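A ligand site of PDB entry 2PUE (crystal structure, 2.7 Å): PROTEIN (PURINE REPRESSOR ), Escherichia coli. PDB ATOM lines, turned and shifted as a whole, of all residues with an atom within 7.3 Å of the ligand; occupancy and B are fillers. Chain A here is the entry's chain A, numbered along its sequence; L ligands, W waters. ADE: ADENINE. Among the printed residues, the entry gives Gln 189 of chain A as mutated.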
ATOM      1  N   THR A  66     -19.270 -20.568  -3.918  1.00  0.00           N
ATOM      2  CA  THR A  66     -19.382 -19.543  -4.949  1.00  0.00           C
ATOM      3  C   THR A  66     -20.808 -19.614  -5.462  1.00  0.00           C
ATOM      4  O   THR A  66     -21.517 -18.628  -5.454  1.00  0.00           O
ATOM      5  CB  THR A  66     -18.426 -19.827  -6.091  1.00  0.00           C
ATOM      6  OG1 THR A  66     -17.153 -19.219  -5.836  1.00  0.00           O
ATOM      7  CG2 THR A  66     -18.972 -19.285  -7.350  1.00  0.00           C
ATOM      8  N   SER A  67     -21.210 -20.803  -5.877  1.00  0.00           N
ATOM      9  CA  SER A  67     -22.560 -21.037  -6.369  1.00  0.00           C
ATOM     10  C   SER A  67     -22.850 -22.448  -5.979  1.00  0.00           C
ATOM     11  O   SER A  67     -21.950 -23.181  -5.609  1.00  0.00           O
ATOM     12  CB  SER A  67     -22.614 -20.895  -7.904  1.00  0.00           C
ATOM     13  OG  SER A  67     -23.544 -21.811  -8.495  1.00  0.00           O
ATOM     14  N   ALA A  70     -24.737 -25.028 -10.298  1.00  0.00           N
ATOM     15  CA  ALA A  70     -23.885 -25.664 -11.305  1.00  0.00           C
ATOM     16  C   ALA A  70     -23.557 -27.056 -10.878  1.00  0.00           C
ATOM     17  O   ALA A  70     -22.958 -27.302  -9.767  1.00  0.00           O
ATOM     18  CB  ALA A  70     -22.589 -24.876 -11.508  1.00  0.00           C
ATOM     19  N   ALA A  71     -23.963 -27.965 -11.757  1.00  0.00           N
ATOM     20  CA  ALA A  71     -23.740 -29.382 -11.599  1.00  0.00           C
ATOM     21  C   ALA A  71     -22.474 -29.701 -10.750  1.00  0.00           C
ATOM     22  O   ALA A  71     -22.568 -30.296  -9.704  1.00  0.00           O
ATOM     23  CB  ALA A  71     -23.655 -30.045 -12.966  1.00  0.00           C
ATOM     24  N   TYR A  72     -21.336 -29.227 -11.230  1.00  0.00           N
ATOM     25  CA  TYR A  72     -20.063 -29.429 -10.592  1.00  0.00           C
ATOM     26  C   TYR A  72     -20.204 -29.160  -9.111  1.00  0.00           C
ATOM     27  O   TYR A  72     -20.313 -30.108  -8.277  1.00  0.00           O
ATOM     28  CB  TYR A  72     -19.055 -28.506 -11.254  1.00  0.00           C
ATOM     29  CG  TYR A  72     -17.659 -28.581 -10.740  1.00  0.00           C
ATOM     30  CD1 TYR A  72     -17.255 -27.743  -9.717  1.00  0.00           C
ATOM     31  CD2 TYR A  72     -16.726 -29.411 -11.312  1.00  0.00           C
ATOM     32  CE1 TYR A  72     -15.974 -27.760  -9.255  1.00  0.00           C
ATOM     33  CE2 TYR A  72     -15.431 -29.428 -10.851  1.00  0.00           C
ATOM     34  CZ  TYR A  72     -15.069 -28.600  -9.813  1.00  0.00           C
ATOM     35  OH  TYR A  72     -13.801 -28.584  -9.339  1.00  0.00           O
ATOM     36  N   PHE A  73     -20.330 -27.882  -8.798  1.00  0.00           N
ATOM     37  CA  PHE A  73     -20.523 -27.414  -7.423  1.00  0.00           C
ATOM     38  C   PHE A  73     -21.497 -28.254  -6.671  1.00  0.00           C
ATOM     39  O   PHE A  73     -21.240 -28.718  -5.554  1.00  0.00           O
ATOM     40  CB  PHE A  73     -21.060 -26.033  -7.472  1.00  0.00           C
ATOM     41  CG  PHE A  73     -20.039 -25.051  -7.872  1.00  0.00           C
ATOM     42  CD1 PHE A  73     -18.746 -25.201  -7.415  1.00  0.00           C
ATOM     43  CD2 PHE A  73     -20.334 -24.030  -8.736  1.00  0.00           C
ATOM     44  CE1 PHE A  73     -17.795 -24.324  -7.770  1.00  0.00           C
ATOM     45  CE2 PHE A  73     -19.370 -23.129  -9.110  1.00  0.00           C
ATOM     46  CZ  PHE A  73     -18.104 -23.274  -8.633  1.00  0.00           C
ATOM     47  N   SER A 123     -13.594 -20.018  -6.120  1.00  0.00           N
ATOM     48  CA  SER A 123     -13.325 -19.855  -7.552  1.00  0.00           C
ATOM     49  C   SER A 123     -12.189 -18.892  -7.733  1.00  0.00           C
ATOM     50  O   SER A 123     -11.081 -19.299  -8.006  1.00  0.00           O
ATOM     51  CB  SER A 123     -14.577 -19.322  -8.295  1.00  0.00           C
ATOM     52  OG  SER A 123     -15.656 -20.260  -8.259  1.00  0.00           O
ATOM     53  N   ASP A 145     -10.318 -25.586  -3.822  1.00  0.00           N
ATOM     54  CA  ASP A 145     -10.160 -25.304  -5.251  1.00  0.00           C
ATOM     55  C   ASP A 145      -8.927 -24.574  -5.735  1.00  0.00           C
ATOM     56  O   ASP A 145      -9.000 -23.868  -6.752  1.00  0.00           O
ATOM     57  CB  ASP A 145     -11.417 -24.652  -5.830  1.00  0.00           C
ATOM     58  CG  ASP A 145     -11.847 -23.379  -5.064  1.00  0.00           C
ATOM     59  OD1 ASP A 145     -10.972 -22.655  -4.551  1.00  0.00           O
ATOM     60  OD2 ASP A 145     -13.060 -23.067  -5.050  1.00  0.00           O
ATOM     61  N   ASP A 159      -6.437 -30.694  -6.998  1.00  0.00           N
ATOM     62  CA  ASP A 159      -7.004 -31.570  -8.023  1.00  0.00           C
ATOM     63  C   ASP A 159      -6.128 -32.010  -9.170  1.00  0.00           C
ATOM     64  O   ASP A 159      -6.482 -32.921  -9.853  1.00  0.00           O
ATOM     65  CB  ASP A 159      -8.233 -30.918  -8.604  1.00  0.00           C
ATOM     66  CG  ASP A 159      -7.899 -29.666  -9.377  1.00  0.00           C
ATOM     67  OD1 ASP A 159      -6.709 -29.236  -9.339  1.00  0.00           O
ATOM     68  OD2 ASP A 159      -8.788 -29.161 -10.089  1.00  0.00           O
ATOM     69  N   PRO A 186     -12.751 -19.401 -17.254  1.00  0.00           N
ATOM     70  CA  PRO A 186     -12.105 -18.206 -16.634  1.00  0.00           C
ATOM     71  C   PRO A 186     -10.659 -18.454 -16.209  1.00  0.00           C
ATOM     72  O   PRO A 186     -10.390 -19.302 -15.360  1.00  0.00           O
ATOM     73  CB  PRO A 186     -12.974 -17.945 -15.416  1.00  0.00           C
ATOM     74  CG  PRO A 186     -14.239 -18.843 -15.580  1.00  0.00           C
ATOM     75  CD  PRO A 186     -13.817 -19.983 -16.424  1.00  0.00           C
ATOM     76  N   GLN A 189      -9.464 -18.746 -12.598  1.00  0.00           N
ATOM     77  CA  GLN A 189      -9.719 -19.927 -11.807  1.00  0.00           C
ATOM     78  C   GLN A 189      -8.693 -21.008 -12.125  1.00  0.00           C
ATOM     79  O   GLN A 189      -8.106 -21.052 -13.223  1.00  0.00           O
ATOM     80  CB  GLN A 189     -11.138 -20.444 -12.028  1.00  0.00           C
ATOM     81  CG  GLN A 189     -12.184 -19.350 -12.003  1.00  0.00           C
ATOM     82  CD  GLN A 189     -13.553 -19.894 -11.741  1.00  0.00           C
ATOM     83  OE1 GLN A 189     -13.700 -21.078 -11.380  1.00  0.00           O
ATOM     84  NE2 GLN A 189     -14.584 -19.050 -11.927  1.00  0.00           N
ATOM     85  N   ASN A 190      -8.482 -21.870 -11.145  1.00  0.00           N
ATOM     86  CA  ASN A 190      -7.575 -22.975 -11.284  1.00  0.00           C
ATOM     87  C   ASN A 190      -8.064 -23.914 -12.431  1.00  0.00           C
ATOM     88  O   ASN A 190      -7.318 -24.194 -13.377  1.00  0.00           O
ATOM     89  CB  ASN A 190      -7.517 -23.743  -9.969  1.00  0.00           C
ATOM     90  CG  ASN A 190      -6.847 -25.077 -10.116  1.00  0.00           C
ATOM     91  OD1 ASN A 190      -5.780 -25.173 -10.745  1.00  0.00           O
ATOM     92  ND2 ASN A 190      -7.557 -26.156  -9.694  1.00  0.00           N
ATOM     93  N   THR A 191      -9.318 -24.373 -12.313  1.00  0.00           N
ATOM     94  CA  THR A 191      -9.940 -25.254 -13.304  1.00  0.00           C
ATOM     95  C   THR A 191      -9.951 -24.577 -14.658  1.00  0.00           C
ATOM     96  O   THR A 191     -10.274 -25.197 -15.664  1.00  0.00           O
ATOM     97  CB  THR A 191     -11.401 -25.622 -12.941  1.00  0.00           C
ATOM     98  OG1 THR A 191     -12.039 -24.488 -12.355  1.00  0.00           O
ATOM     99  CG2 THR A 191     -11.433 -26.770 -11.931  1.00  0.00           C
ATOM    100  N   GLY A 192      -9.603 -23.295 -14.672  1.00  0.00           N
ATOM    101  CA  GLY A 192      -9.544 -22.550 -15.914  1.00  0.00           C
ATOM    102  C   GLY A 192      -8.102 -22.582 -16.423  1.00  0.00           C
ATOM    103  O   GLY A 192      -7.727 -23.408 -17.270  1.00  0.00           O
ATOM    104  N   ARG A 195      -6.263 -26.342 -16.185  1.00  0.00           N
ATOM    105  CA  ARG A 195      -6.619 -27.316 -17.193  1.00  0.00           C
ATOM    106  C   ARG A 195      -6.027 -26.930 -18.589  1.00  0.00           C
ATOM    107  O   ARG A 195      -5.374 -27.735 -19.258  1.00  0.00           O
ATOM    108  CB  ARG A 195      -8.152 -27.476 -17.239  1.00  0.00           C
ATOM    109  CG  ARG A 195      -8.762 -28.174 -15.983  1.00  0.00           C
ATOM    110  CD  ARG A 195     -10.309 -28.109 -15.936  1.00  0.00           C
ATOM    111  NE  ARG A 195     -10.864 -28.745 -14.721  1.00  0.00           N
ATOM    112  CZ  ARG A 195     -12.169 -28.843 -14.442  1.00  0.00           C
ATOM    113  NH1 ARG A 195     -13.086 -28.368 -15.289  1.00  0.00           N
ATOM    114  NH2 ARG A 195     -12.556 -29.428 -13.312  1.00  0.00           N
ATOM    115  N   ASP A 219     -17.312 -19.530 -19.437  1.00  0.00           N
ATOM    116  CA  ASP A 219     -17.456 -19.179 -18.031  1.00  0.00           C
ATOM    117  C   ASP A 219     -18.002 -20.360 -17.266  1.00  0.00           C
ATOM    118  O   ASP A 219     -18.379 -20.230 -16.099  1.00  0.00           O
ATOM    119  CB  ASP A 219     -18.410 -17.978 -17.884  1.00  0.00           C
ATOM    120  CG  ASP A 219     -19.803 -18.234 -18.534  1.00  0.00           C
ATOM    121  OD1 ASP A 219     -20.306 -19.372 -18.533  1.00  0.00           O
ATOM    122  OD2 ASP A 219     -20.413 -17.253 -18.988  1.00  0.00           O
ATOM    123  N   PHE A 220     -18.112 -21.489 -17.963  1.00  0.00           N
ATOM    124  CA  PHE A 220     -18.626 -22.741 -17.398  1.00  0.00           C
ATOM    125  C   PHE A 220     -20.094 -22.931 -17.553  1.00  0.00           C
ATOM    126  O   PHE A 220     -20.601 -23.979 -17.203  1.00  0.00           O
ATOM    127  CB  PHE A 220     -18.271 -22.953 -15.932  1.00  0.00           C
ATOM    128  CG  PHE A 220     -16.826 -23.229 -15.686  1.00  0.00           C
ATOM    129  CD1 PHE A 220     -16.189 -24.297 -16.301  1.00  0.00           C
ATOM    130  CD2 PHE A 220     -16.096 -22.436 -14.801  1.00  0.00           C
ATOM    131  CE1 PHE A 220     -14.850 -24.554 -16.066  1.00  0.00           C
ATOM    132  CE2 PHE A 220     -14.779 -22.686 -14.567  1.00  0.00           C
ATOM    133  CZ  PHE A 220     -14.149 -23.753 -15.203  1.00  0.00           C
ATOM    134  N   GLU A 221     -20.790 -21.932 -18.049  1.00  0.00           N
ATOM    135  CA  GLU A 221     -22.237 -22.062 -18.222  1.00  0.00           C
ATOM    136  C   GLU A 221     -22.533 -22.445 -19.639  1.00  0.00           C
ATOM    137  O   GLU A 221     -21.842 -21.986 -20.593  1.00  0.00           O
ATOM    138  CB  GLU A 221     -22.947 -20.751 -17.869  1.00  0.00           C
ATOM    139  CG  GLU A 221     -22.713 -20.270 -16.446  1.00  0.00           C
ATOM    140  CD  GLU A 221     -23.877 -20.564 -15.505  1.00  0.00           C
ATOM    141  OE1 GLU A 221     -23.892 -21.656 -14.896  1.00  0.00           O
ATOM    142  OE2 GLU A 221     -24.727 -19.662 -15.301  1.00  0.00           O
ATOM    143  N   GLY A 245     -13.315 -26.996 -21.591  1.00  0.00           N
ATOM    144  CA  GLY A 245     -12.959 -26.900 -20.180  1.00  0.00           C
ATOM    145  C   GLY A 245     -13.914 -27.411 -19.095  1.00  0.00           C
ATOM    146  O   GLY A 245     -13.508 -27.551 -17.921  1.00  0.00           O
ATOM    147  N   GLY A 246     -15.172 -27.635 -19.448  1.00  0.00           N
ATOM    148  CA  GLY A 246     -16.195 -28.110 -18.474  1.00  0.00           C
ATOM    149  C   GLY A 246     -17.349 -28.864 -19.193  1.00  0.00           C
ATOM    150  O   GLY A 246     -17.689 -28.568 -20.362  1.00  0.00           O
ATOM    151  N   ASP A 247     -17.946 -29.825 -18.509  1.00  0.00           N
ATOM    152  CA  ASP A 247     -19.016 -30.594 -19.103  1.00  0.00           C
ATOM    153  C   ASP A 247     -20.250 -29.784 -19.540  1.00  0.00           C
ATOM    154  O   ASP A 247     -20.688 -29.867 -20.722  1.00  0.00           O
ATOM    155  CB  ASP A 247     -19.367 -31.757 -18.249  1.00  0.00           C
ATOM    156  CG  ASP A 247     -18.276 -32.830 -18.251  1.00  0.00           C
ATOM    157  OD1 ASP A 247     -17.242 -32.619 -18.912  1.00  0.00           O
ATOM    158  OD2 ASP A 247     -18.496 -33.902 -17.648  1.00  0.00           O
ATOM    159  N   ILE A 248     -20.808 -29.000 -18.631  1.00  0.00           N
ATOM    160  CA  ILE A 248     -21.959 -28.168 -18.964  1.00  0.00           C
ATOM    161  C   ILE A 248     -21.702 -27.314 -20.236  1.00  0.00           C
ATOM    162  O   ILE A 248     -22.435 -27.424 -21.229  1.00  0.00           O
ATOM    163  CB  ILE A 248     -22.378 -27.293 -17.837  1.00  0.00           C
ATOM    164  CG1 ILE A 248     -22.478 -28.098 -16.545  1.00  0.00           C
ATOM    165  CG2 ILE A 248     -23.688 -26.642 -18.184  1.00  0.00           C
ATOM    166  CD1 ILE A 248     -23.648 -29.077 -16.472  1.00  0.00           C
ATOM    167  N   TYR A 273     -14.648 -31.892 -19.671  1.00  0.00           N
ATOM    168  CA  TYR A 273     -13.928 -32.000 -18.439  1.00  0.00           C
ATOM    169  C   TYR A 273     -14.812 -31.829 -17.226  1.00  0.00           C
ATOM    170  O   TYR A 273     -15.480 -30.804 -17.107  1.00  0.00           O
ATOM    171  CB  TYR A 273     -12.859 -30.957 -18.410  1.00  0.00           C
ATOM    172  CG  TYR A 273     -11.757 -31.274 -17.450  1.00  0.00           C
ATOM    173  CD1 TYR A 273     -12.029 -31.692 -16.165  1.00  0.00           C
ATOM    174  CD2 TYR A 273     -10.421 -31.140 -17.834  1.00  0.00           C
ATOM    175  CE1 TYR A 273     -11.015 -31.943 -15.281  1.00  0.00           C
ATOM    176  CE2 TYR A 273      -9.406 -31.377 -16.954  1.00  0.00           C
ATOM    177  CZ  TYR A 273      -9.701 -31.793 -15.690  1.00  0.00           C
ATOM    178  OH  TYR A 273      -8.687 -32.060 -14.812  1.00  0.00           O
ATOM    179  N   ASP A 274     -14.777 -32.836 -16.342  1.00  0.00           N
ATOM    180  CA  ASP A 274     -15.497 -32.897 -15.042  1.00  0.00           C
ATOM    181  C   ASP A 274     -16.135 -34.246 -14.849  1.00  0.00           C
ATOM    182  O   ASP A 274     -16.101 -34.832 -13.771  1.00  0.00           O
ATOM    183  CB  ASP A 274     -16.603 -31.823 -14.904  1.00  0.00           C
ATOM    184  CG  ASP A 274     -16.042 -30.415 -14.495  1.00  0.00           C
ATOM    185  OD1 ASP A 274     -14.834 -30.227 -14.452  1.00  0.00           O
ATOM    186  OD2 ASP A 274     -16.831 -29.448 -14.531  1.00  0.00           O
ATOM    187  N   VAL A 276     -19.495 -34.962 -15.044  1.00  0.00           N
ATOM    188  CA  VAL A 276     -20.590 -34.673 -14.146  1.00  0.00           C
ATOM    189  C   VAL A 276     -21.556 -35.809 -14.215  1.00  0.00           C
ATOM    190  O   VAL A 276     -21.683 -36.440 -15.259  1.00  0.00           O
ATOM    191  CB  VAL A 276     -21.295 -33.399 -14.604  1.00  0.00           C
ATOM    192  CG1 VAL A 276     -22.785 -33.579 -14.615  1.00  0.00           C
ATOM    193  CG2 VAL A 276     -20.844 -32.217 -13.742  1.00  0.00           C
ATOM    194  N   GLN A 291     -13.181 -35.830 -12.647  1.00  0.00           N
ATOM    195  CA  GLN A 291     -12.643 -35.257 -11.420  1.00  0.00           C
ATOM    196  C   GLN A 291     -13.346 -36.003 -10.333  1.00  0.00           C
ATOM    197  O   GLN A 291     -14.542 -36.243 -10.405  1.00  0.00           O
ATOM    198  CB  GLN A 291     -13.014 -33.778 -11.277  1.00  0.00           C
ATOM    199  CG  GLN A 291     -12.466 -33.109  -9.994  1.00  0.00           C
ATOM    200  CD  GLN A 291     -11.389 -32.014 -10.282  1.00  0.00           C
ATOM    201  OE1 GLN A 291     -11.617 -30.828 -10.032  1.00  0.00           O
ATOM    202  NE2 GLN A 291     -10.219 -32.430 -10.743  1.00  0.00           N
HETATM  203  N9  ADE L   1     -15.665 -27.400 -13.281  1.00  0.00           N
HETATM  204  C8  ADE L   1     -14.475 -26.948 -12.771  1.00  0.00           C
HETATM  205  N7  ADE L   1     -14.569 -25.781 -12.199  1.00  0.00           N
HETATM  206  C5  ADE L   1     -15.903 -25.432 -12.367  1.00  0.00           C
HETATM  207  C6  ADE L   1     -16.599 -24.282 -11.959  1.00  0.00           C
HETATM  208  N6  ADE L   1     -16.061 -23.225 -11.336  1.00  0.00           N
HETATM  209  N1  ADE L   1     -17.945 -24.305 -12.302  1.00  0.00           N
HETATM  210  C2  ADE L   1     -18.548 -25.362 -12.953  1.00  0.00           C
HETATM  211  N3  ADE L   1     -17.913 -26.464 -13.319  1.00  0.00           N
HETATM  212  C4  ADE L   1     -16.589 -26.428 -13.010  1.00  0.00           C
HETATM  213  O   HOH W   1     -13.019 -25.641  -9.611  1.00  0.00           O
HETATM  214  O   HOH W   2     -17.100 -20.278 -11.042  1.00  0.00           O
HETATM  215  O   HOH W   3     -18.946 -21.574 -12.490  1.00  0.00           O
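Residues that only touch the ligand: Tyr 72, Phe 73 and Phe 220. Hydrophobic or aromatic side chains that line the ligand: Tyr 72, Phe 73 and Phe 220. Seven residues have an atom within 4 Å of the ligand: Tyr 72, Phe 73, Gln 189, Thr 191, Arg 195, Phe 220 and Asp 274. Along chain A the residues within 4 Å of the ligand span positions 72 to 274.
Water W1 lies within hydrogen-bond range of N7 of the ligand (3.0 Å), OH of Tyr 72 (3.1 Å) and OG1 of Thr 191 (3.1 Å). Water W2 lies within hydrogen-bond range of the side-chain amide nitrogen (NE2) of Gln 189 (2.9 Å), the side-chain hydroxyl (OG) of Ser 123 (3.1 Å) and a nitrogen (N6) of the ligand (3.1 Å).
A nitrogen (N9) of the ligand sits at hydrogen-bond distance from the side-chain carboxylate (OD2) of Asp 274 (2.7 Å). The side-chain hydroxyl of Thr 191 sits at hydrogen-bond distance from a nitrogen (N7) of the ligand (2.8 Å). OE1 of Gln 189 lies within hydrogen-bond range of N6 of the ligand (3.2 Å). The guanidinium group of Arg 195 lies close to a nitrogen (N9) of the ligand (3.4 Å).
The guanidinium group (NH1) of Arg 195 sits at hydrogen-bond distance from the backbone carbonyl oxygen (O) of Gly 245, 2.8 Å away. The guanidinium group of Arg 195 lies within salt-bridge range of the side-chain carboxylate of Asp 274 (2.7 Å). The backbone carbonyl oxygen (O) of Asp 274 lies within hydrogen-bond range of the backbone NH (N) of Gln 291. The side-chain amide oxygen (OE1) of Gln 291 lies within hydrogen-bond range of the side-chain hydroxyl (OH) of Tyr 72 (3.2 Å).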
